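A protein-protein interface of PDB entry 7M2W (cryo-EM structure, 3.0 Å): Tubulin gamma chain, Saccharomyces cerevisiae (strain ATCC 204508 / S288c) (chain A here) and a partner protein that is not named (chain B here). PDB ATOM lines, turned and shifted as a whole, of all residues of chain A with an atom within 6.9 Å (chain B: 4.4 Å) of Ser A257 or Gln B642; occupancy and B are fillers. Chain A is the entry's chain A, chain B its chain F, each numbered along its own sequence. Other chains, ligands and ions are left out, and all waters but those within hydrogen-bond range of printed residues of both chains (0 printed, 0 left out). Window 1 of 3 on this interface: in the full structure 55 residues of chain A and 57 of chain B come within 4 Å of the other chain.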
ATOM      1  N   TYR A 249      18.046  -4.444   9.850  1.00  0.00           N
ATOM      2  CA  TYR A 249      18.513  -5.815   9.700  1.00  0.00           C
ATOM      3  C   TYR A 249      18.044  -6.654  10.878  1.00  0.00           C
ATOM      4  O   TYR A 249      18.165  -6.246  12.036  1.00  0.00           O
ATOM      5  CB  TYR A 249      20.042  -5.878   9.588  1.00  0.00           C
ATOM      6  CG  TYR A 249      20.636  -4.814   8.696  1.00  0.00           C
ATOM      7  CD1 TYR A 249      21.220  -3.678   9.236  1.00  0.00           C
ATOM      8  CD2 TYR A 249      20.608  -4.942   7.316  1.00  0.00           C
ATOM      9  CE1 TYR A 249      21.761  -2.703   8.428  1.00  0.00           C
ATOM     10  CE2 TYR A 249      21.147  -3.971   6.500  1.00  0.00           C
ATOM     11  CZ  TYR A 249      21.722  -2.855   7.062  1.00  0.00           C
ATOM     12  OH  TYR A 249      22.261  -1.882   6.254  1.00  0.00           O
ATOM     13  N   MET A 252      20.480 -12.966   9.532  1.00  0.00           N
ATOM     14  CA  MET A 252      21.793 -13.143   8.924  1.00  0.00           C
ATOM     15  C   MET A 252      21.734 -13.022   7.409  1.00  0.00           C
ATOM     16  O   MET A 252      22.718 -12.610   6.786  1.00  0.00           O
ATOM     17  CB  MET A 252      22.379 -14.498   9.312  1.00  0.00           C
ATOM     18  CG  MET A 252      22.717 -14.650  10.775  1.00  0.00           C
ATOM     19  SD  MET A 252      24.058 -13.561  11.273  1.00  0.00           S
ATOM     20  CE  MET A 252      24.244 -14.047  12.981  1.00  0.00           C
ATOM     21  N   SER A 253      20.603 -13.382   6.800  1.00  0.00           N
ATOM     22  CA  SER A 253      20.474 -13.258   5.353  1.00  0.00           C
ATOM     23  C   SER A 253      20.612 -11.808   4.912  1.00  0.00           C
ATOM     24  O   SER A 253      21.304 -11.512   3.932  1.00  0.00           O
ATOM     25  CB  SER A 253      19.134 -13.832   4.895  1.00  0.00           C
ATOM     26  OG  SER A 253      18.950 -15.147   5.388  1.00  0.00           O
ATOM     27  N   SER A 254      19.975 -10.887   5.634  1.00  0.00           N
ATOM     28  CA  SER A 254      20.083  -9.473   5.292  1.00  0.00           C
ATOM     29  C   SER A 254      21.496  -8.955   5.521  1.00  0.00           C
ATOM     30  O   SER A 254      22.048  -8.247   4.672  1.00  0.00           O
ATOM     31  CB  SER A 254      19.078  -8.662   6.104  1.00  0.00           C
ATOM     32  OG  SER A 254      19.232  -8.918   7.488  1.00  0.00           O
ATOM     33  N   ILE A 255      22.091  -9.292   6.667  1.00  0.00           N
ATOM     34  CA  ILE A 255      23.458  -8.868   6.959  1.00  0.00           C
ATOM     35  C   ILE A 255      24.409  -9.350   5.872  1.00  0.00           C
ATOM     36  O   ILE A 255      25.327  -8.631   5.461  1.00  0.00           O
ATOM     37  CB  ILE A 255      23.885  -9.375   8.348  1.00  0.00           C
ATOM     38  CG1 ILE A 255      23.208  -8.562   9.449  1.00  0.00           C
ATOM     39  CG2 ILE A 255      25.393  -9.314   8.506  1.00  0.00           C
ATOM     40  CD1 ILE A 255      23.682  -8.918  10.838  1.00  0.00           C
ATOM     41  N   TYR A 256      24.199 -10.568   5.378  1.00  0.00           N
ATOM     42  CA  TYR A 256      25.128 -11.132   4.409  1.00  0.00           C
ATOM     43  C   TYR A 256      24.872 -10.617   2.999  1.00  0.00           C
ATOM     44  O   TYR A 256      25.822 -10.458   2.227  1.00  0.00           O
ATOM     45  CB  TYR A 256      25.078 -12.657   4.477  1.00  0.00           C
ATOM     46  CG  TYR A 256      25.730 -13.167   5.742  1.00  0.00           C
ATOM     47  CD1 TYR A 256      25.502 -14.455   6.204  1.00  0.00           C
ATOM     48  CD2 TYR A 256      26.569 -12.345   6.482  1.00  0.00           C
ATOM     49  CE1 TYR A 256      26.098 -14.906   7.370  1.00  0.00           C
ATOM     50  CE2 TYR A 256      27.164 -12.784   7.641  1.00  0.00           C
ATOM     51  CZ  TYR A 256      26.929 -14.063   8.082  1.00  0.00           C
ATOM     52  OH  TYR A 256      27.534 -14.486   9.242  1.00  0.00           O
ATOM     53  N   SER A 257      23.615 -10.344   2.640  1.00  0.00           N
ATOM     54  CA  SER A 257      23.368  -9.633   1.390  1.00  0.00           C
ATOM     55  C   SER A 257      23.940  -8.226   1.448  1.00  0.00           C
ATOM     56  O   SER A 257      24.265  -7.640   0.409  1.00  0.00           O
ATOM     57  CB  SER A 257      21.872  -9.581   1.095  1.00  0.00           C
ATOM     58  OG  SER A 257      21.266  -8.482   1.752  1.00  0.00           O
ATOM     59  N   THR A 258      24.063  -7.672   2.653  1.00  0.00           N
ATOM     60  CA  THR A 258      24.803  -6.431   2.840  1.00  0.00           C
ATOM     61  C   THR A 258      26.293  -6.641   2.603  1.00  0.00           C
ATOM     62  O   THR A 258      26.949  -5.833   1.935  1.00  0.00           O
ATOM     63  CB  THR A 258      24.551  -5.892   4.249  1.00  0.00           C
ATOM     64  OG1 THR A 258      23.175  -5.515   4.384  1.00  0.00           O
ATOM     65  CG2 THR A 258      25.447  -4.714   4.550  1.00  0.00           C
ATOM     66  N   LEU A 259      26.844  -7.728   3.145  1.00  0.00           N
ATOM     67  CA  LEU A 259      28.287  -7.934   3.117  1.00  0.00           C
ATOM     68  C   LEU A 259      28.755  -8.712   1.895  1.00  0.00           C
ATOM     69  O   LEU A 259      29.767  -8.342   1.289  1.00  0.00           O
ATOM     70  CB  LEU A 259      28.734  -8.652   4.387  1.00  0.00           C
ATOM     71  CG  LEU A 259      29.089  -7.729   5.548  1.00  0.00           C
ATOM     72  CD1 LEU A 259      29.198  -8.506   6.839  1.00  0.00           C
ATOM     73  CD2 LEU A 259      30.389  -7.017   5.252  1.00  0.00           C
ATOM     74  N   ILE A 260      28.062  -9.781   1.521  1.00  0.00           N
ATOM     75  CA  ILE A 260      28.556 -10.695   0.492  1.00  0.00           C
ATOM     76  C   ILE A 260      28.079 -10.248  -0.883  1.00  0.00           C
ATOM     77  O   ILE A 260      26.886 -10.373  -1.193  1.00  0.00           O
ATOM     78  CB  ILE A 260      28.114 -12.140   0.770  1.00  0.00           C
ATOM     79  CG1 ILE A 260      28.620 -12.613   2.136  1.00  0.00           C
ATOM     80  CG2 ILE A 260      28.592 -13.063  -0.335  1.00  0.00           C
ATOM     81  CD1 ILE A 260      30.012 -12.153   2.482  1.00  0.00           C
ATOM     82  N   PRO A 261      28.961  -9.722  -1.738  1.00  0.00           N
ATOM     83  CA  PRO A 261      28.528  -9.381  -3.098  1.00  0.00           C
ATOM     84  C   PRO A 261      28.367 -10.592  -3.997  1.00  0.00           C
ATOM     85  O   PRO A 261      27.376 -10.679  -4.733  1.00  0.00           O
ATOM     86  CB  PRO A 261      29.641  -8.450  -3.590  1.00  0.00           C
ATOM     87  CG  PRO A 261      30.855  -8.928  -2.871  1.00  0.00           C
ATOM     88  CD  PRO A 261      30.398  -9.472  -1.539  1.00  0.00           C
ATOM     89  N   ASN A 317      33.069  -4.567   0.364  1.00  0.00           N
ATOM     90  CA  ASN A 317      31.839  -4.235   1.072  1.00  0.00           C
ATOM     91  C   ASN A 317      32.173  -4.068   2.543  1.00  0.00           C
ATOM     92  O   ASN A 317      32.924  -4.870   3.103  1.00  0.00           O
ATOM     93  CB  ASN A 317      30.773  -5.313   0.882  1.00  0.00           C
ATOM     94  CG  ASN A 317      30.006  -5.145  -0.408  1.00  0.00           C
ATOM     95  OD1 ASN A 317      29.451  -4.082  -0.676  1.00  0.00           O
ATOM     96  ND2 ASN A 317      29.963  -6.196  -1.213  1.00  0.00           N
ATOM     97  N   SER A 350      28.164   1.208  -4.736  1.00  0.00           N
ATOM     98  CA  SER A 350      27.571   1.442  -3.436  1.00  0.00           C
ATOM     99  C   SER A 350      28.697   1.701  -2.432  1.00  0.00           C
ATOM    100  O   SER A 350      29.869   1.818  -2.834  1.00  0.00           O
ATOM    101  CB  SER A 350      26.675   0.261  -3.075  1.00  0.00           C
ATOM    102  OG  SER A 350      25.578   0.165  -3.965  1.00  0.00           O
ATOM    103  N   HIS A 353      27.714   0.226   4.592  1.00  0.00           N
ATOM    104  CA  HIS A 353      26.435   0.120   5.278  1.00  0.00           C
ATOM    105  C   HIS A 353      26.661   0.288   6.772  1.00  0.00           C
ATOM    106  O   HIS A 353      27.578  -0.314   7.338  1.00  0.00           O
ATOM    107  CB  HIS A 353      25.765  -1.223   4.998  1.00  0.00           C
ATOM    108  CG  HIS A 353      25.360  -1.411   3.571  1.00  0.00           C
ATOM    109  ND1 HIS A 353      24.173  -0.931   3.064  1.00  0.00           N
ATOM    110  CD2 HIS A 353      25.986  -2.029   2.542  1.00  0.00           C
ATOM    111  CE1 HIS A 353      24.082  -1.245   1.785  1.00  0.00           C
ATOM    112  NE2 HIS A 353      25.171  -1.911   1.443  1.00  0.00           N
ATOM    113  N   ASN B 597      13.062  -6.215  -0.494  1.00  0.00           N
ATOM    114  CA  ASN B 597      13.974  -6.880   0.431  1.00  0.00           C
ATOM    115  C   ASN B 597      13.704  -8.378   0.494  1.00  0.00           C
ATOM    116  O   ASN B 597      14.632  -9.197   0.422  1.00  0.00           O
ATOM    117  CB  ASN B 597      13.841  -6.249   1.817  1.00  0.00           C
ATOM    118  CG  ASN B 597      15.073  -6.442   2.669  1.00  0.00           C
ATOM    119  OD1 ASN B 597      16.091  -6.955   2.202  1.00  0.00           O
ATOM    120  ND2 ASN B 597      14.989  -6.034   3.928  1.00  0.00           N
ATOM    121  N   TYR B 600      14.743 -10.090  -2.716  1.00  0.00           N
ATOM    122  CA  TYR B 600      16.193 -10.149  -2.857  1.00  0.00           C
ATOM    123  C   TYR B 600      16.794 -11.222  -1.965  1.00  0.00           C
ATOM    124  O   TYR B 600      17.716 -11.926  -2.379  1.00  0.00           O
ATOM    125  CB  TYR B 600      16.826  -8.795  -2.551  1.00  0.00           C
ATOM    126  CG  TYR B 600      16.990  -7.946  -3.779  1.00  0.00           C
ATOM    127  CD1 TYR B 600      16.263  -6.785  -3.939  1.00  0.00           C
ATOM    128  CD2 TYR B 600      17.844  -8.331  -4.799  1.00  0.00           C
ATOM    129  CE1 TYR B 600      16.401  -6.017  -5.057  1.00  0.00           C
ATOM    130  CE2 TYR B 600      17.985  -7.567  -5.931  1.00  0.00           C
ATOM    131  CZ  TYR B 600      17.259  -6.409  -6.053  1.00  0.00           C
ATOM    132  OH  TYR B 600      17.378  -5.634  -7.178  1.00  0.00           O
ATOM    133  N   MET B 604      18.705 -14.360  -3.450  1.00  0.00           N
ATOM    134  CA  MET B 604      20.070 -14.565  -2.990  1.00  0.00           C
ATOM    135  C   MET B 604      20.286 -16.011  -2.591  1.00  0.00           C
ATOM    136  O   MET B 604      21.250 -16.649  -3.024  1.00  0.00           O
ATOM    137  CB  MET B 604      20.386 -13.657  -1.804  1.00  0.00           C
ATOM    138  CG  MET B 604      21.726 -13.991  -1.168  1.00  0.00           C
ATOM    139  SD  MET B 604      22.242 -12.872   0.139  1.00  0.00           S
ATOM    140  CE  MET B 604      21.518 -13.675   1.563  1.00  0.00           C
ATOM    141  N   ARG B 638      23.108  -8.010  -8.683  1.00  0.00           N
ATOM    142  CA  ARG B 638      22.032  -8.101  -7.705  1.00  0.00           C
ATOM    143  C   ARG B 638      22.442  -7.470  -6.385  1.00  0.00           C
ATOM    144  O   ARG B 638      21.635  -6.799  -5.732  1.00  0.00           O
ATOM    145  CB  ARG B 638      21.635  -9.562  -7.492  1.00  0.00           C
ATOM    146  CG  ARG B 638      20.800  -9.791  -6.245  1.00  0.00           C
ATOM    147  CD  ARG B 638      20.699 -11.260  -5.879  1.00  0.00           C
ATOM    148  NE  ARG B 638      21.963 -11.799  -5.389  1.00  0.00           N
ATOM    149  CZ  ARG B 638      22.406 -11.652  -4.144  1.00  0.00           C
ATOM    150  NH1 ARG B 638      21.690 -10.974  -3.259  1.00  0.00           N
ATOM    151  NH2 ARG B 638      23.569 -12.179  -3.786  1.00  0.00           N
ATOM    152  N   THR B 639      23.693  -7.678  -5.971  1.00  0.00           N
ATOM    153  CA  THR B 639      24.152  -7.086  -4.722  1.00  0.00           C
ATOM    154  C   THR B 639      24.199  -5.571  -4.815  1.00  0.00           C
ATOM    155  O   THR B 639      23.837  -4.880  -3.863  1.00  0.00           O
ATOM    156  CB  THR B 639      25.522  -7.634  -4.337  1.00  0.00           C
ATOM    157  OG1 THR B 639      25.445  -9.056  -4.196  1.00  0.00           O
ATOM    158  CG2 THR B 639      25.964  -7.025  -3.018  1.00  0.00           C
ATOM    159  N   GLN B 640      24.638  -5.031  -5.953  1.00  0.00           N
ATOM    160  CA  GLN B 640      24.631  -3.577  -6.106  1.00  0.00           C
ATOM    161  C   GLN B 640      23.212  -3.025  -6.029  1.00  0.00           C
ATOM    162  O   GLN B 640      22.962  -2.005  -5.367  1.00  0.00           O
ATOM    163  CB  GLN B 640      25.294  -3.175  -7.423  1.00  0.00           C
ATOM    164  CG  GLN B 640      26.787  -2.919  -7.309  1.00  0.00           C
ATOM    165  CD  GLN B 640      27.351  -2.213  -8.524  1.00  0.00           C
ATOM    166  OE1 GLN B 640      26.611  -1.801  -9.415  1.00  0.00           O
ATOM    167  NE2 GLN B 640      28.670  -2.068  -8.565  1.00  0.00           N
ATOM    168  N   PHE B 641      22.265  -3.706  -6.679  1.00  0.00           N
ATOM    169  CA  PHE B 641      20.867  -3.292  -6.593  1.00  0.00           C
ATOM    170  C   PHE B 641      20.371  -3.305  -5.155  1.00  0.00           C
ATOM    171  O   PHE B 641      19.811  -2.315  -4.670  1.00  0.00           O
ATOM    172  CB  PHE B 641      19.983  -4.204  -7.438  1.00  0.00           C
ATOM    173  CG  PHE B 641      19.809  -3.757  -8.851  1.00  0.00           C
ATOM    174  CD1 PHE B 641      20.860  -3.216  -9.560  1.00  0.00           C
ATOM    175  CD2 PHE B 641      18.572  -3.845  -9.459  1.00  0.00           C
ATOM    176  CE1 PHE B 641      20.688  -2.809 -10.863  1.00  0.00           C
ATOM    177  CE2 PHE B 641      18.393  -3.426 -10.755  1.00  0.00           C
ATOM    178  CZ  PHE B 641      19.450  -2.910 -11.458  1.00  0.00           C
ATOM    179  N   GLN B 642      20.560  -4.427  -4.461  1.00  0.00           N
ATOM    180  CA  GLN B 642      20.036  -4.557  -3.109  1.00  0.00           C
ATOM    181  C   GLN B 642      20.778  -3.647  -2.144  1.00  0.00           C
ATOM    182  O   GLN B 642      20.235  -3.259  -1.108  1.00  0.00           O
ATOM    183  CB  GLN B 642      20.114  -6.013  -2.649  1.00  0.00           C
ATOM    184  CG  GLN B 642      19.492  -6.268  -1.289  1.00  0.00           C
ATOM    185  CD  GLN B 642      19.694  -7.690  -0.817  1.00  0.00           C
ATOM    186  OE1 GLN B 642      19.238  -8.068   0.262  1.00  0.00           O
ATOM    187  NE2 GLN B 642      20.378  -8.490  -1.626  1.00  0.00           N
ATOM    188  N   GLN B 643      22.006  -3.259  -2.481  1.00  0.00           N
ATOM    189  CA  GLN B 643      22.728  -2.323  -1.632  1.00  0.00           C
ATOM    190  C   GLN B 643      22.180  -0.916  -1.785  1.00  0.00           C
ATOM    191  O   GLN B 643      22.026  -0.199  -0.793  1.00  0.00           O
ATOM    192  CB  GLN B 643      24.221  -2.366  -1.947  1.00  0.00           C
ATOM    193  CG  GLN B 643      24.937  -3.547  -1.322  1.00  0.00           C
ATOM    194  CD  GLN B 643      26.429  -3.521  -1.559  1.00  0.00           C
ATOM    195  OE1 GLN B 643      26.915  -2.867  -2.481  1.00  0.00           O
ATOM    196  NE2 GLN B 643      27.166  -4.233  -0.721  1.00  0.00           N
ATOM    197  N   PHE B 644      21.861  -0.502  -3.014  1.00  0.00           N
ATOM    198  CA  PHE B 644      21.143   0.760  -3.178  1.00  0.00           C
ATOM    199  C   PHE B 644      19.808   0.718  -2.444  1.00  0.00           C
ATOM    200  O   PHE B 644      19.415   1.683  -1.774  1.00  0.00           O
ATOM    201  CB  PHE B 644      20.925   1.065  -4.661  1.00  0.00           C
ATOM    202  CG  PHE B 644      19.758   1.976  -4.923  1.00  0.00           C
ATOM    203  CD1 PHE B 644      19.896   3.345  -4.810  1.00  0.00           C
ATOM    204  CD2 PHE B 644      18.523   1.461  -5.282  1.00  0.00           C
ATOM    205  CE1 PHE B 644      18.828   4.186  -5.048  1.00  0.00           C
ATOM    206  CE2 PHE B 644      17.452   2.296  -5.522  1.00  0.00           C
ATOM    207  CZ  PHE B 644      17.605   3.659  -5.403  1.00  0.00           C
ATOM    208  N   ASN B 645      19.099  -0.405  -2.566  1.00  0.00           N
ATOM    209  CA  ASN B 645      17.815  -0.573  -1.892  1.00  0.00           C
ATOM    210  C   ASN B 645      17.958  -0.442  -0.383  1.00  0.00           C
ATOM    211  O   ASN B 645      17.170   0.244   0.274  1.00  0.00           O
ATOM    212  CB  ASN B 645      17.227  -1.935  -2.254  1.00  0.00           C
ATOM    213  CG  ASN B 645      15.788  -2.071  -1.844  1.00  0.00           C
ATOM    214  OD1 ASN B 645      15.139  -1.096  -1.477  1.00  0.00           O
ATOM    215  ND2 ASN B 645      15.284  -3.291  -1.879  1.00  0.00           N
ATOM    216  N   SER B 646      18.969  -1.098   0.183  1.00  0.00           N
ATOM    217  CA  SER B 646      19.169  -1.073   1.625  1.00  0.00           C
ATOM    218  C   SER B 646      19.652   0.291   2.087  1.00  0.00           C
ATOM    219  O   SER B 646      19.321   0.721   3.193  1.00  0.00           O
ATOM    220  CB  SER B 646      20.157  -2.163   2.033  1.00  0.00           C
ATOM    221  OG  SER B 646      20.400  -2.134   3.427  1.00  0.00           O
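The guanidinium group (NH1) of Arg B638 lies close to the side-chain amide nitrogen (NE2) of Gln B642 (3.2 Å).
ND2 of Asn A317 lies close to O of Leu A259 (3.3 Å).
The backbone carbonyl oxygen (O) of Ser A254 lies within hydrogen-bond range of the side-chain hydroxyl (OG) of Ser A257 (3.0 Å).
The backbone carbonyl oxygen of Ser A254 is in hydrogen-bond range of the side-chain hydroxyl of Thr A258 (3.0 Å).
Of chain A, only Ser A257 comes within 4 Å of Gln B642.
Of the printed residues of chain B, Asn A317 touches Gln B643 (2.3 Å).
Of the printed residues of chain B, Ser A350 touches Gln B640 (3.7 Å), Gln B643 (3.2 Å) and Phe B644 (3.9 Å).
Printed residues of chain B within 4 Å of Ile A260: Thr B639.
Of the printed residues of chain B, Thr A258 touches Gln B643 (3.1 Å).
Of the printed residues of chain A, Phe B644 touches Ser A350 (3.9 Å).
Ser A253 touches Met B604 (O to CE, 3.2 Å).
Ser A257 touches Met B604 (CB to SD, 3.4 Å).
Ser A257 touches Thr B639.
OG1 of Thr B639 touches O of Ile A260 (3.6 Å).
Ser A350 touches Gln B640.
CB of Ser A350 touches OE1 of Gln B643, at 3.2 Å.
Ser A350 touches Phe B644 (OG to N, 3.9 Å).
NE2 of His A353 touches CG of Gln B643 (3.2 Å).
Ser B646 touches His A353.
Hydrophobic or aromatic side chains of chain B that line the printed part of chain A: Met B604.
Hydrophobic or aromatic side chains of chain A that line the printed part of chain B: Tyr A249, Pro A261 and His A353.
Among the printed residues, no Asp or Glu carboxylate lies within 4 Å of a Lys or Arg side-chain nitrogen of the other chain.
The side-chain amide oxygen (OE1) of Gln B643 lies close to the side-chain amide oxygen (OD1) of Asn A317 (3.3 Å).
The side-chain hydroxyl of Tyr A249 sits at hydrogen-bond distance from the side-chain hydroxyl of Ser B646.
The side-chain amide nitrogen (NE2) of Gln B643 sits at hydrogen-bond distance from the backbone carbonyl oxygen (O) of Thr A258 (3.1 Å).
OG of Ser A257 is in hydrogen-bond range of OE1 of Gln B642 (2.6 Å).
The side-chain hydroxyl (OG1) of Thr B639 sits at hydrogen-bond distance from the backbone carbonyl oxygen (O) of Pro A261 (2.6 Å).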
